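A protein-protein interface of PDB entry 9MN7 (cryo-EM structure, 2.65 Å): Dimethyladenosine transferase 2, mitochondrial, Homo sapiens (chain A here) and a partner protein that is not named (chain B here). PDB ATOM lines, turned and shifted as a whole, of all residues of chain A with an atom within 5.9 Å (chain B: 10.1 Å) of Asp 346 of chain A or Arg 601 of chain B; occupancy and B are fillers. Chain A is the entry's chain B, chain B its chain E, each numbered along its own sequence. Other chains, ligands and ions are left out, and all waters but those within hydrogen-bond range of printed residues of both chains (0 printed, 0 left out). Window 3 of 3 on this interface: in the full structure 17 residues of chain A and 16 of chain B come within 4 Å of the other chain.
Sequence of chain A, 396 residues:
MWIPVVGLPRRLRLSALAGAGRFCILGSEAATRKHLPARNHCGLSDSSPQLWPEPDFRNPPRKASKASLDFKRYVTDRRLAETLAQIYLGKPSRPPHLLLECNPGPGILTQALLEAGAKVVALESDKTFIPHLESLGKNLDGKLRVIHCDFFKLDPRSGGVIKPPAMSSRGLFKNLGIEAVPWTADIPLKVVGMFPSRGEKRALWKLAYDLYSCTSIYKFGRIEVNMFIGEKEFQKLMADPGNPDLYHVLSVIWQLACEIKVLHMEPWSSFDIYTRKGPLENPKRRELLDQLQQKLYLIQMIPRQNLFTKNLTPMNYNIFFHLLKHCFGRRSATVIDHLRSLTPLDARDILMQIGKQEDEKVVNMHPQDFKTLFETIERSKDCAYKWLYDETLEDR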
ATOM      1  N   ARG A 340     -28.217   6.628  15.909  1.00  0.00           N
ATOM      2  CA  ARG A 340     -26.930   7.293  15.701  1.00  0.00           C
ATOM      3  C   ARG A 340     -25.751   6.429  16.131  1.00  0.00           C
ATOM      4  O   ARG A 340     -24.642   6.621  15.625  1.00  0.00           O
ATOM      5  CB  ARG A 340     -26.873   8.639  16.430  1.00  0.00           C
ATOM      6  CG  ARG A 340     -27.303   9.833  15.584  1.00  0.00           C
ATOM      7  CD  ARG A 340     -28.800   9.900  15.416  1.00  0.00           C
ATOM      8  NE  ARG A 340     -29.221  11.032  14.600  1.00  0.00           N
ATOM      9  CZ  ARG A 340     -29.453  12.248  15.072  1.00  0.00           C
ATOM     10  NH1 ARG A 340     -29.298  12.533  16.355  1.00  0.00           N
ATOM     11  NH2 ARG A 340     -29.849  13.203  14.237  1.00  0.00           N
ATOM     12  N   PRO A 344     -25.875   5.853  10.087  1.00  0.00           N
ATOM     13  CA  PRO A 344     -25.495   7.235   9.781  1.00  0.00           C
ATOM     14  C   PRO A 344     -26.628   8.097   9.249  1.00  0.00           C
ATOM     15  O   PRO A 344     -26.397   9.276   8.954  1.00  0.00           O
ATOM     16  CB  PRO A 344     -24.410   7.053   8.716  1.00  0.00           C
ATOM     17  CG  PRO A 344     -24.806   5.816   8.011  1.00  0.00           C
ATOM     18  CD  PRO A 344     -25.421   4.914   9.047  1.00  0.00           C
ATOM     19  N   LEU A 345     -27.831   7.548   9.105  1.00  0.00           N
ATOM     20  CA  LEU A 345     -28.961   8.333   8.637  1.00  0.00           C
ATOM     21  C   LEU A 345     -29.496   9.231   9.747  1.00  0.00           C
ATOM     22  O   LEU A 345     -29.232   9.027  10.935  1.00  0.00           O
ATOM     23  CB  LEU A 345     -30.079   7.432   8.123  1.00  0.00           C
ATOM     24  CG  LEU A 345     -29.714   6.674   6.853  1.00  0.00           C
ATOM     25  CD1 LEU A 345     -30.827   5.740   6.429  1.00  0.00           C
ATOM     26  CD2 LEU A 345     -29.401   7.666   5.758  1.00  0.00           C
ATOM     27  N   ASP A 346     -30.257  10.242   9.334  1.00  0.00           N
ATOM     28  CA  ASP A 346     -30.955  11.099  10.281  1.00  0.00           C
ATOM     29  C   ASP A 346     -32.021  10.277  10.992  1.00  0.00           C
ATOM     30  O   ASP A 346     -33.005   9.859  10.375  1.00  0.00           O
ATOM     31  CB  ASP A 346     -31.583  12.283   9.545  1.00  0.00           C
ATOM     32  CG  ASP A 346     -32.125  13.355  10.484  1.00  0.00           C
ATOM     33  OD1 ASP A 346     -32.052  13.198  11.722  1.00  0.00           O
ATOM     34  OD2 ASP A 346     -32.639  14.370   9.972  1.00  0.00           O
ATOM     35  N   ALA A 347     -31.807  10.031  12.288  1.00  0.00           N
ATOM     36  CA  ALA A 347     -32.714   9.168  13.036  1.00  0.00           C
ATOM     37  C   ALA A 347     -34.084   9.808  13.204  1.00  0.00           C
ATOM     38  O   ALA A 347     -35.102   9.115  13.132  1.00  0.00           O
ATOM     39  CB  ALA A 347     -32.123   8.828  14.398  1.00  0.00           C
ATOM     40  N   ARG A 348     -34.129  11.124  13.430  1.00  0.00           N
ATOM     41  CA  ARG A 348     -35.412  11.802  13.589  1.00  0.00           C
ATOM     42  C   ARG A 348     -36.228  11.761  12.302  1.00  0.00           C
ATOM     43  O   ARG A 348     -37.461  11.693  12.353  1.00  0.00           O
ATOM     44  CB  ARG A 348     -35.188  13.242  14.051  1.00  0.00           C
ATOM     45  CG  ARG A 348     -36.439  13.932  14.568  1.00  0.00           C
ATOM     46  CD  ARG A 348     -36.133  15.324  15.096  1.00  0.00           C
ATOM     47  NE  ARG A 348     -37.316  15.962  15.661  1.00  0.00           N
ATOM     48  CZ  ARG A 348     -37.341  17.190  16.161  1.00  0.00           C
ATOM     49  NH1 ARG A 348     -36.259  17.951  16.181  1.00  0.00           N
ATOM     50  NH2 ARG A 348     -38.480  17.667  16.655  1.00  0.00           N
ATOM     51  N   ASP A 349     -35.559  11.756  11.145  1.00  0.00           N
ATOM     52  CA  ASP A 349     -36.258  11.563   9.879  1.00  0.00           C
ATOM     53  C   ASP A 349     -36.841  10.157   9.776  1.00  0.00           C
ATOM     54  O   ASP A 349     -37.969   9.982   9.300  1.00  0.00           O
ATOM     55  CB  ASP A 349     -35.315  11.842   8.712  1.00  0.00           C
ATOM     56  CG  ASP A 349     -35.876  11.378   7.385  1.00  0.00           C
ATOM     57  OD1 ASP A 349     -37.009  11.778   7.048  1.00  0.00           O
ATOM     58  OD2 ASP A 349     -35.184  10.614   6.679  1.00  0.00           O
ATOM     59  N   ILE A 350     -36.098   9.147  10.237  1.00  0.00           N
ATOM     60  CA  ILE A 350     -36.602   7.774  10.228  1.00  0.00           C
ATOM     61  C   ILE A 350     -37.790   7.635  11.176  1.00  0.00           C
ATOM     62  O   ILE A 350     -38.765   6.927  10.885  1.00  0.00           O
ATOM     63  CB  ILE A 350     -35.465   6.793  10.579  1.00  0.00           C
ATOM     64  CG1 ILE A 350     -34.324   6.918   9.568  1.00  0.00           C
ATOM     65  CG2 ILE A 350     -35.964   5.353  10.613  1.00  0.00           C
ATOM     66  CD1 ILE A 350     -33.131   6.040   9.882  1.00  0.00           C
ATOM     67  N   LEU A 351     -37.743   8.337  12.308  1.00  0.00           N
ATOM     68  CA  LEU A 351     -38.843   8.274  13.265  1.00  0.00           C
ATOM     69  C   LEU A 351     -40.067   9.044  12.786  1.00  0.00           C
ATOM     70  O   LEU A 351     -41.201   8.659  13.090  1.00  0.00           O
ATOM     71  CB  LEU A 351     -38.387   8.752  14.644  1.00  0.00           C
ATOM     72  CG  LEU A 351     -37.757   7.714  15.580  1.00  0.00           C
ATOM     73  CD1 LEU A 351     -38.821   6.687  15.909  1.00  0.00           C
ATOM     74  CD2 LEU A 351     -36.540   7.006  15.044  1.00  0.00           C
ATOM     75  N   LEU B 437     -10.732  18.117   4.899  1.00  0.00           N
ATOM     76  CA  LEU B 437     -11.395  17.574   6.079  1.00  0.00           C
ATOM     77  C   LEU B 437     -10.444  17.490   7.265  1.00  0.00           C
ATOM     78  O   LEU B 437     -10.832  17.788   8.398  1.00  0.00           O
ATOM     79  CB  LEU B 437     -11.979  16.198   5.765  1.00  0.00           C
ATOM     80  CG  LEU B 437     -13.320  16.161   5.033  1.00  0.00           C
ATOM     81  CD1 LEU B 437     -13.822  14.733   4.936  1.00  0.00           C
ATOM     82  CD2 LEU B 437     -14.338  17.043   5.727  1.00  0.00           C
ATOM     83  N   GLN B 588     -16.165  15.830  12.622  1.00  0.00           N
ATOM     84  CA  GLN B 588     -17.443  15.749  11.930  1.00  0.00           C
ATOM     85  C   GLN B 588     -17.190  15.840  10.434  1.00  0.00           C
ATOM     86  O   GLN B 588     -16.375  16.653   9.991  1.00  0.00           O
ATOM     87  CB  GLN B 588     -18.393  16.866  12.379  1.00  0.00           C
ATOM     88  CG  GLN B 588     -19.128  16.591  13.680  1.00  0.00           C
ATOM     89  CD  GLN B 588     -19.941  17.782  14.143  1.00  0.00           C
ATOM     90  OE1 GLN B 588     -19.966  18.821  13.484  1.00  0.00           O
ATOM     91  NE2 GLN B 588     -20.622  17.634  15.273  1.00  0.00           N
ATOM     92  N   MET B 589     -17.889  15.010   9.664  1.00  0.00           N
ATOM     93  CA  MET B 589     -17.732  14.998   8.220  1.00  0.00           C
ATOM     94  C   MET B 589     -19.082  15.201   7.535  1.00  0.00           C
ATOM     95  O   MET B 589     -20.128  14.910   8.123  1.00  0.00           O
ATOM     96  CB  MET B 589     -17.108  13.676   7.749  1.00  0.00           C
ATOM     97  CG  MET B 589     -17.967  12.447   7.987  1.00  0.00           C
ATOM     98  SD  MET B 589     -17.188  10.932   7.402  1.00  0.00           S
ATOM     99  CE  MET B 589     -17.330  11.144   5.634  1.00  0.00           C
ATOM    100  N   PRO B 590     -19.102  15.733   6.311  1.00  0.00           N
ATOM    101  CA  PRO B 590     -20.365  15.772   5.559  1.00  0.00           C
ATOM    102  C   PRO B 590     -20.827  14.365   5.208  1.00  0.00           C
ATOM    103  O   PRO B 590     -20.030  13.514   4.807  1.00  0.00           O
ATOM    104  CB  PRO B 590     -20.025  16.589   4.306  1.00  0.00           C
ATOM    105  CG  PRO B 590     -18.558  16.706   4.261  1.00  0.00           C
ATOM    106  CD  PRO B 590     -18.005  16.429   5.617  1.00  0.00           C
ATOM    107  N   CYS B 591     -22.130  14.125   5.381  1.00  0.00           N
ATOM    108  CA  CYS B 591     -22.679  12.790   5.169  1.00  0.00           C
ATOM    109  C   CYS B 591     -22.707  12.426   3.690  1.00  0.00           C
ATOM    110  O   CYS B 591     -22.408  11.284   3.321  1.00  0.00           O
ATOM    111  CB  CYS B 591     -24.082  12.703   5.766  1.00  0.00           C
ATOM    112  SG  CYS B 591     -25.255  13.892   5.078  1.00  0.00           S
ATOM    113  N   SER B 592     -23.062  13.376   2.833  1.00  0.00           N
ATOM    114  CA  SER B 592     -23.182  13.134   1.398  1.00  0.00           C
ATOM    115  C   SER B 592     -21.924  13.659   0.714  1.00  0.00           C
ATOM    116  O   SER B 592     -21.803  14.855   0.443  1.00  0.00           O
ATOM    117  CB  SER B 592     -24.439  13.795   0.842  1.00  0.00           C
ATOM    118  OG  SER B 592     -24.220  15.169   0.581  1.00  0.00           O
ATOM    119  N   LEU B 593     -20.987  12.756   0.438  1.00  0.00           N
ATOM    120  CA  LEU B 593     -19.788  13.084  -0.320  1.00  0.00           C
ATOM    121  C   LEU B 593     -19.965  12.873  -1.816  1.00  0.00           C
ATOM    122  O   LEU B 593     -19.007  13.070  -2.572  1.00  0.00           O
ATOM    123  CB  LEU B 593     -18.602  12.251   0.179  1.00  0.00           C
ATOM    124  CG  LEU B 593     -18.109  12.524   1.599  1.00  0.00           C
ATOM    125  CD1 LEU B 593     -16.876  11.690   1.904  1.00  0.00           C
ATOM    126  CD2 LEU B 593     -17.813  14.003   1.784  1.00  0.00           C
ATOM    127  N   ASP B 594     -21.158  12.464  -2.254  1.00  0.00           N
ATOM    128  CA  ASP B 594     -21.410  12.275  -3.679  1.00  0.00           C
ATOM    129  C   ASP B 594     -21.403  13.601  -4.430  1.00  0.00           C
ATOM    130  O   ASP B 594     -20.841  13.697  -5.527  1.00  0.00           O
ATOM    131  CB  ASP B 594     -22.737  11.539  -3.879  1.00  0.00           C
ATOM    132  CG  ASP B 594     -23.865  12.117  -3.038  1.00  0.00           C
ATOM    133  OD1 ASP B 594     -23.635  13.117  -2.325  1.00  0.00           O
ATOM    134  OD2 ASP B 594     -24.985  11.570  -3.091  1.00  0.00           O
ATOM    135  N   LYS B 595     -22.021  14.633  -3.860  1.00  0.00           N
ATOM    136  CA  LYS B 595     -22.061  15.958  -4.467  1.00  0.00           C
ATOM    137  C   LYS B 595     -21.470  16.966  -3.492  1.00  0.00           C
ATOM    138  O   LYS B 595     -22.049  17.188  -2.415  1.00  0.00           O
ATOM    139  CB  LYS B 595     -23.489  16.369  -4.856  1.00  0.00           C
ATOM    140  CG  LYS B 595     -24.085  15.672  -6.089  1.00  0.00           C
ATOM    141  CD  LYS B 595     -24.615  14.271  -5.806  1.00  0.00           C
ATOM    142  CE  LYS B 595     -25.249  13.659  -7.044  1.00  0.00           C
ATOM    143  NZ  LYS B 595     -25.799  12.302  -6.773  1.00  0.00           N
ATOM    144  N   PRO B 596     -20.325  17.582  -3.805  1.00  0.00           N
ATOM    145  CA  PRO B 596     -19.770  18.598  -2.895  1.00  0.00           C
ATOM    146  C   PRO B 596     -20.608  19.862  -2.815  1.00  0.00           C
ATOM    147  O   PRO B 596     -20.617  20.517  -1.765  1.00  0.00           O
ATOM    148  CB  PRO B 596     -18.381  18.880  -3.486  1.00  0.00           C
ATOM    149  CG  PRO B 596     -18.485  18.471  -4.919  1.00  0.00           C
ATOM    150  CD  PRO B 596     -19.441  17.317  -4.953  1.00  0.00           C
ATOM    151  N   ARG B 598     -23.834  19.969  -2.854  1.00  0.00           N
ATOM    152  CA  ARG B 598     -25.043  19.690  -2.093  1.00  0.00           C
ATOM    153  C   ARG B 598     -24.846  20.031  -0.621  1.00  0.00           C
ATOM    154  O   ARG B 598     -23.770  19.815  -0.054  1.00  0.00           O
ATOM    155  CB  ARG B 598     -25.432  18.220  -2.238  1.00  0.00           C
ATOM    156  CG  ARG B 598     -26.535  17.956  -3.249  1.00  0.00           C
ATOM    157  CD  ARG B 598     -27.095  16.552  -3.084  1.00  0.00           C
ATOM    158  NE  ARG B 598     -28.038  16.207  -4.141  1.00  0.00           N
ATOM    159  CZ  ARG B 598     -28.641  15.032  -4.251  1.00  0.00           C
ATOM    160  NH1 ARG B 598     -28.423  14.058  -3.382  1.00  0.00           N
ATOM    161  NH2 ARG B 598     -29.485  14.826  -5.259  1.00  0.00           N
ATOM    162  N   SER B 599     -25.895  20.565  -0.002  1.00  0.00           N
ATOM    163  CA  SER B 599     -25.885  20.857   1.424  1.00  0.00           C
ATOM    164  C   SER B 599     -26.125  19.561   2.188  1.00  0.00           C
ATOM    165  O   SER B 599     -27.119  18.867   1.946  1.00  0.00           O
ATOM    166  CB  SER B 599     -26.947  21.898   1.775  1.00  0.00           C
ATOM    167  OG  SER B 599     -28.235  21.466   1.371  1.00  0.00           O
ATOM    168  N   SER B 600     -25.214  19.234   3.100  1.00  0.00           N
ATOM    169  CA  SER B 600     -25.263  17.983   3.841  1.00  0.00           C
ATOM    170  C   SER B 600     -25.110  18.263   5.327  1.00  0.00           C
ATOM    171  O   SER B 600     -24.314  19.120   5.724  1.00  0.00           O
ATOM    172  CB  SER B 600     -24.169  17.025   3.367  1.00  0.00           C
ATOM    173  OG  SER B 600     -22.929  17.701   3.267  1.00  0.00           O
ATOM    174  N   ARG B 601     -25.877  17.545   6.140  1.00  0.00           N
ATOM    175  CA  ARG B 601     -25.722  17.614   7.584  1.00  0.00           C
ATOM    176  C   ARG B 601     -24.425  16.934   8.008  1.00  0.00           C
ATOM    177  O   ARG B 601     -23.846  16.130   7.272  1.00  0.00           O
ATOM    178  CB  ARG B 601     -26.922  16.970   8.273  1.00  0.00           C
ATOM    179  CG  ARG B 601     -26.879  15.462   8.273  1.00  0.00           C
ATOM    180  CD  ARG B 601     -28.275  14.858   8.280  1.00  0.00           C
ATOM    181  NE  ARG B 601     -28.229  13.454   7.891  1.00  0.00           N
ATOM    182  CZ  ARG B 601     -27.731  12.474   8.632  1.00  0.00           C
ATOM    183  NH1 ARG B 601     -27.408  12.658   9.902  1.00  0.00           N
ATOM    184  NH2 ARG B 601     -27.568  11.274   8.089  1.00  0.00           N
ATOM    185  N   LEU B 602     -23.959  17.279   9.203  1.00  0.00           N
ATOM    186  CA  LEU B 602     -22.662  16.811   9.669  1.00  0.00           C
ATOM    187  C   LEU B 602     -22.836  15.574  10.541  1.00  0.00           C
ATOM    188  O   LEU B 602     -23.582  15.596  11.524  1.00  0.00           O
ATOM    189  CB  LEU B 602     -21.937  17.912  10.443  1.00  0.00           C
ATOM    190  CG  LEU B 602     -21.139  18.993   9.692  1.00  0.00           C
ATOM    191  CD1 LEU B 602     -19.974  18.375   8.931  1.00  0.00           C
ATOM    192  CD2 LEU B 602     -21.984  19.870   8.769  1.00  0.00           C
ATOM    193  N   VAL B 603     -22.146  14.500  10.179  1.00  0.00           N
ATOM    194  CA  VAL B 603     -22.240  13.236  10.904  1.00  0.00           C
ATOM    195  C   VAL B 603     -20.901  12.956  11.577  1.00  0.00           C
ATOM    196  O   VAL B 603     -19.861  13.446  11.108  1.00  0.00           O
ATOM    197  CB  VAL B 603     -22.658  12.094   9.964  1.00  0.00           C
ATOM    198  CG1 VAL B 603     -24.059  12.337   9.442  1.00  0.00           C
ATOM    199  CG2 VAL B 603     -21.686  11.979   8.806  1.00  0.00           C
ATOM    200  N   PRO B 604     -20.875  12.224  12.691  1.00  0.00           N
ATOM    201  CA  PRO B 604     -19.592  11.888  13.317  1.00  0.00           C
ATOM    202  C   PRO B 604     -18.747  10.983  12.434  1.00  0.00           C
ATOM    203  O   PRO B 604     -19.257  10.103  11.736  1.00  0.00           O
ATOM    204  CB  PRO B 604     -20.002  11.178  14.613  1.00  0.00           C
ATOM    205  CG  PRO B 604     -21.389  11.641  14.880  1.00  0.00           C
ATOM    206  CD  PRO B 604     -22.016  11.829  13.536  1.00  0.00           C
ATOM    207  N   VAL B 605     -17.436  11.223  12.463  1.00  0.00           N
ATOM    208  CA  VAL B 605     -16.497  10.349  11.768  1.00  0.00           C
ATOM    209  C   VAL B 605     -16.414   8.988  12.447  1.00  0.00           C
ATOM    210  O   VAL B 605     -16.291   7.963  11.764  1.00  0.00           O
ATOM    211  CB  VAL B 605     -15.119  11.031  11.684  1.00  0.00           C
ATOM    212  CG1 VAL B 605     -14.097  10.150  10.980  1.00  0.00           C
ATOM    213  CG2 VAL B 605     -15.236  12.368  10.980  1.00  0.00           C
ATOM    214  N   TYR B 607     -18.131   6.173  15.374  1.00  0.00           N
ATOM    215  CA  TYR B 607     -19.376   5.785  16.022  1.00  0.00           C
ATOM    216  C   TYR B 607     -19.106   4.747  17.097  1.00  0.00           C
ATOM    217  O   TYR B 607     -18.202   3.919  16.965  1.00  0.00           O
ATOM    218  CB  TYR B 607     -20.414   5.208  15.045  1.00  0.00           C
ATOM    219  CG  TYR B 607     -20.799   6.073  13.862  1.00  0.00           C
ATOM    220  CD1 TYR B 607     -19.943   6.263  12.781  1.00  0.00           C
ATOM    221  CD2 TYR B 607     -22.034   6.698  13.829  1.00  0.00           C
ATOM    222  CE1 TYR B 607     -20.315   7.052  11.709  1.00  0.00           C
ATOM    223  CE2 TYR B 607     -22.411   7.487  12.770  1.00  0.00           C
ATOM    224  CZ  TYR B 607     -21.552   7.661  11.713  1.00  0.00           C
ATOM    225  OH  TYR B 607     -21.942   8.451  10.661  1.00  0.00           O
ATOM    226  N   HIS B 624     -16.780   5.923   9.897  1.00  0.00           N
ATOM    227  CA  HIS B 624     -17.829   6.080   8.904  1.00  0.00           C
ATOM    228  C   HIS B 624     -17.414   5.339   7.634  1.00  0.00           C
ATOM    229  O   HIS B 624     -16.245   5.409   7.235  1.00  0.00           O
ATOM    230  CB  HIS B 624     -18.042   7.571   8.620  1.00  0.00           C
ATOM    231  CG  HIS B 624     -19.306   7.898   7.879  1.00  0.00           C
ATOM    232  ND1 HIS B 624     -19.687   7.273   6.714  1.00  0.00           N
ATOM    233  CD2 HIS B 624     -20.257   8.830   8.128  1.00  0.00           C
ATOM    234  CE1 HIS B 624     -20.829   7.782   6.289  1.00  0.00           C
ATOM    235  NE2 HIS B 624     -21.195   8.732   7.130  1.00  0.00           N
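Of chain A, only Pro 344, Leu 345 and Asp 346 come within 4 Å of Arg 601 of chain B.
Of chain B, only Arg 601 comes within 4 Å of Leu 345 of chain A.
No residue of chain B comes within 4 Å of Ala 347 of chain A.
No residue of chain B comes within 4 Å of Asp 349 of chain A.
Of the printed residues of chain B, Pro 344 of chain A touches Arg 601, Val 603, Tyr 607 and His 624.
Printed residues of chain B within 4 Å of Arg 340 of chain A: Tyr 607 (3.2 Å).
Of the printed residues of chain A, Tyr 607 of chain B touches Arg 340 (3.2 Å) and Pro 344 (3.4 Å).
Ile 350 of chain A touches none of the printed residues of chain B.
The nearest residue of chain B that does not touch Asp 346 of chain A is Val 603 of chain B (6.5 Å).
The nearest residue of chain A that does not touch Arg 601 of chain B is Arg 340 of chain A (5.0 Å).
Of the 20 printed residues of chain B, 4 touch a printed residue of chain A.
Printed residues of chain B that touch a printed residue of chain A: Arg 601, Val 603, Tyr 607 and His 624.
Hydrophobic or aromatic side chains of chain A that line the printed part of chain B: Pro 344.
Among the printed residues, no Asp or Glu carboxylate lies within 4 Å of a Lys or Arg side-chain nitrogen of the other chain.
The guanidinium group of Arg 340 of chain A lies within salt-bridge range of the side-chain carboxylate of Asp 346 of chain A (3.3 Å).
OD1 of Asp 346 of chain A sits close to N of Arg 348 of chain A (3.4 Å).
The backbone NH of Met 589 of chain B lies within hydrogen-bond range of the backbone carbonyl oxygen of Val 603 of chain B (2.9 Å).
The backbone NH (N) of Cys 591 of chain B sits at hydrogen-bond distance from the backbone carbonyl oxygen (O) of Arg 601 of chain B, at 3.2 Å.
The backbone carbonyl oxygen (O) of Pro 604 of chain B lies close to the side-chain hydroxyl (OH) of Tyr 607 of chain B (3.3 Å).
The backbone NH (N) of His 624 of chain B lies within hydrogen-bond range of the backbone carbonyl oxygen (O) of Val 605 of chain B.
Tyr 607 of chain B touches Arg 340 of chain A (CD2 to O, 3.2 Å).
Pro 344 of chain A touches Val 603 of chain B.
Pro 344 of chain A touches Tyr 607 of chain B (CB to OH, 3.4 Å).
NE2 of His 624 of chain B touches CB of Pro 344 of chain A, at 3.96 Å.
Leu 345 of chain A touches Arg 601 of chain B (C to NH2, 3.3 Å).
The guanidinium group (NH2) of Arg 601 of chain B sits at hydrogen-bond distance from the backbone carbonyl oxygen (O) of Pro 344 of chain A (2.5 Å).
NH2 of Arg 601 of chain B lies close to N of Asp 346 of chain A, at 3.1 Å.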
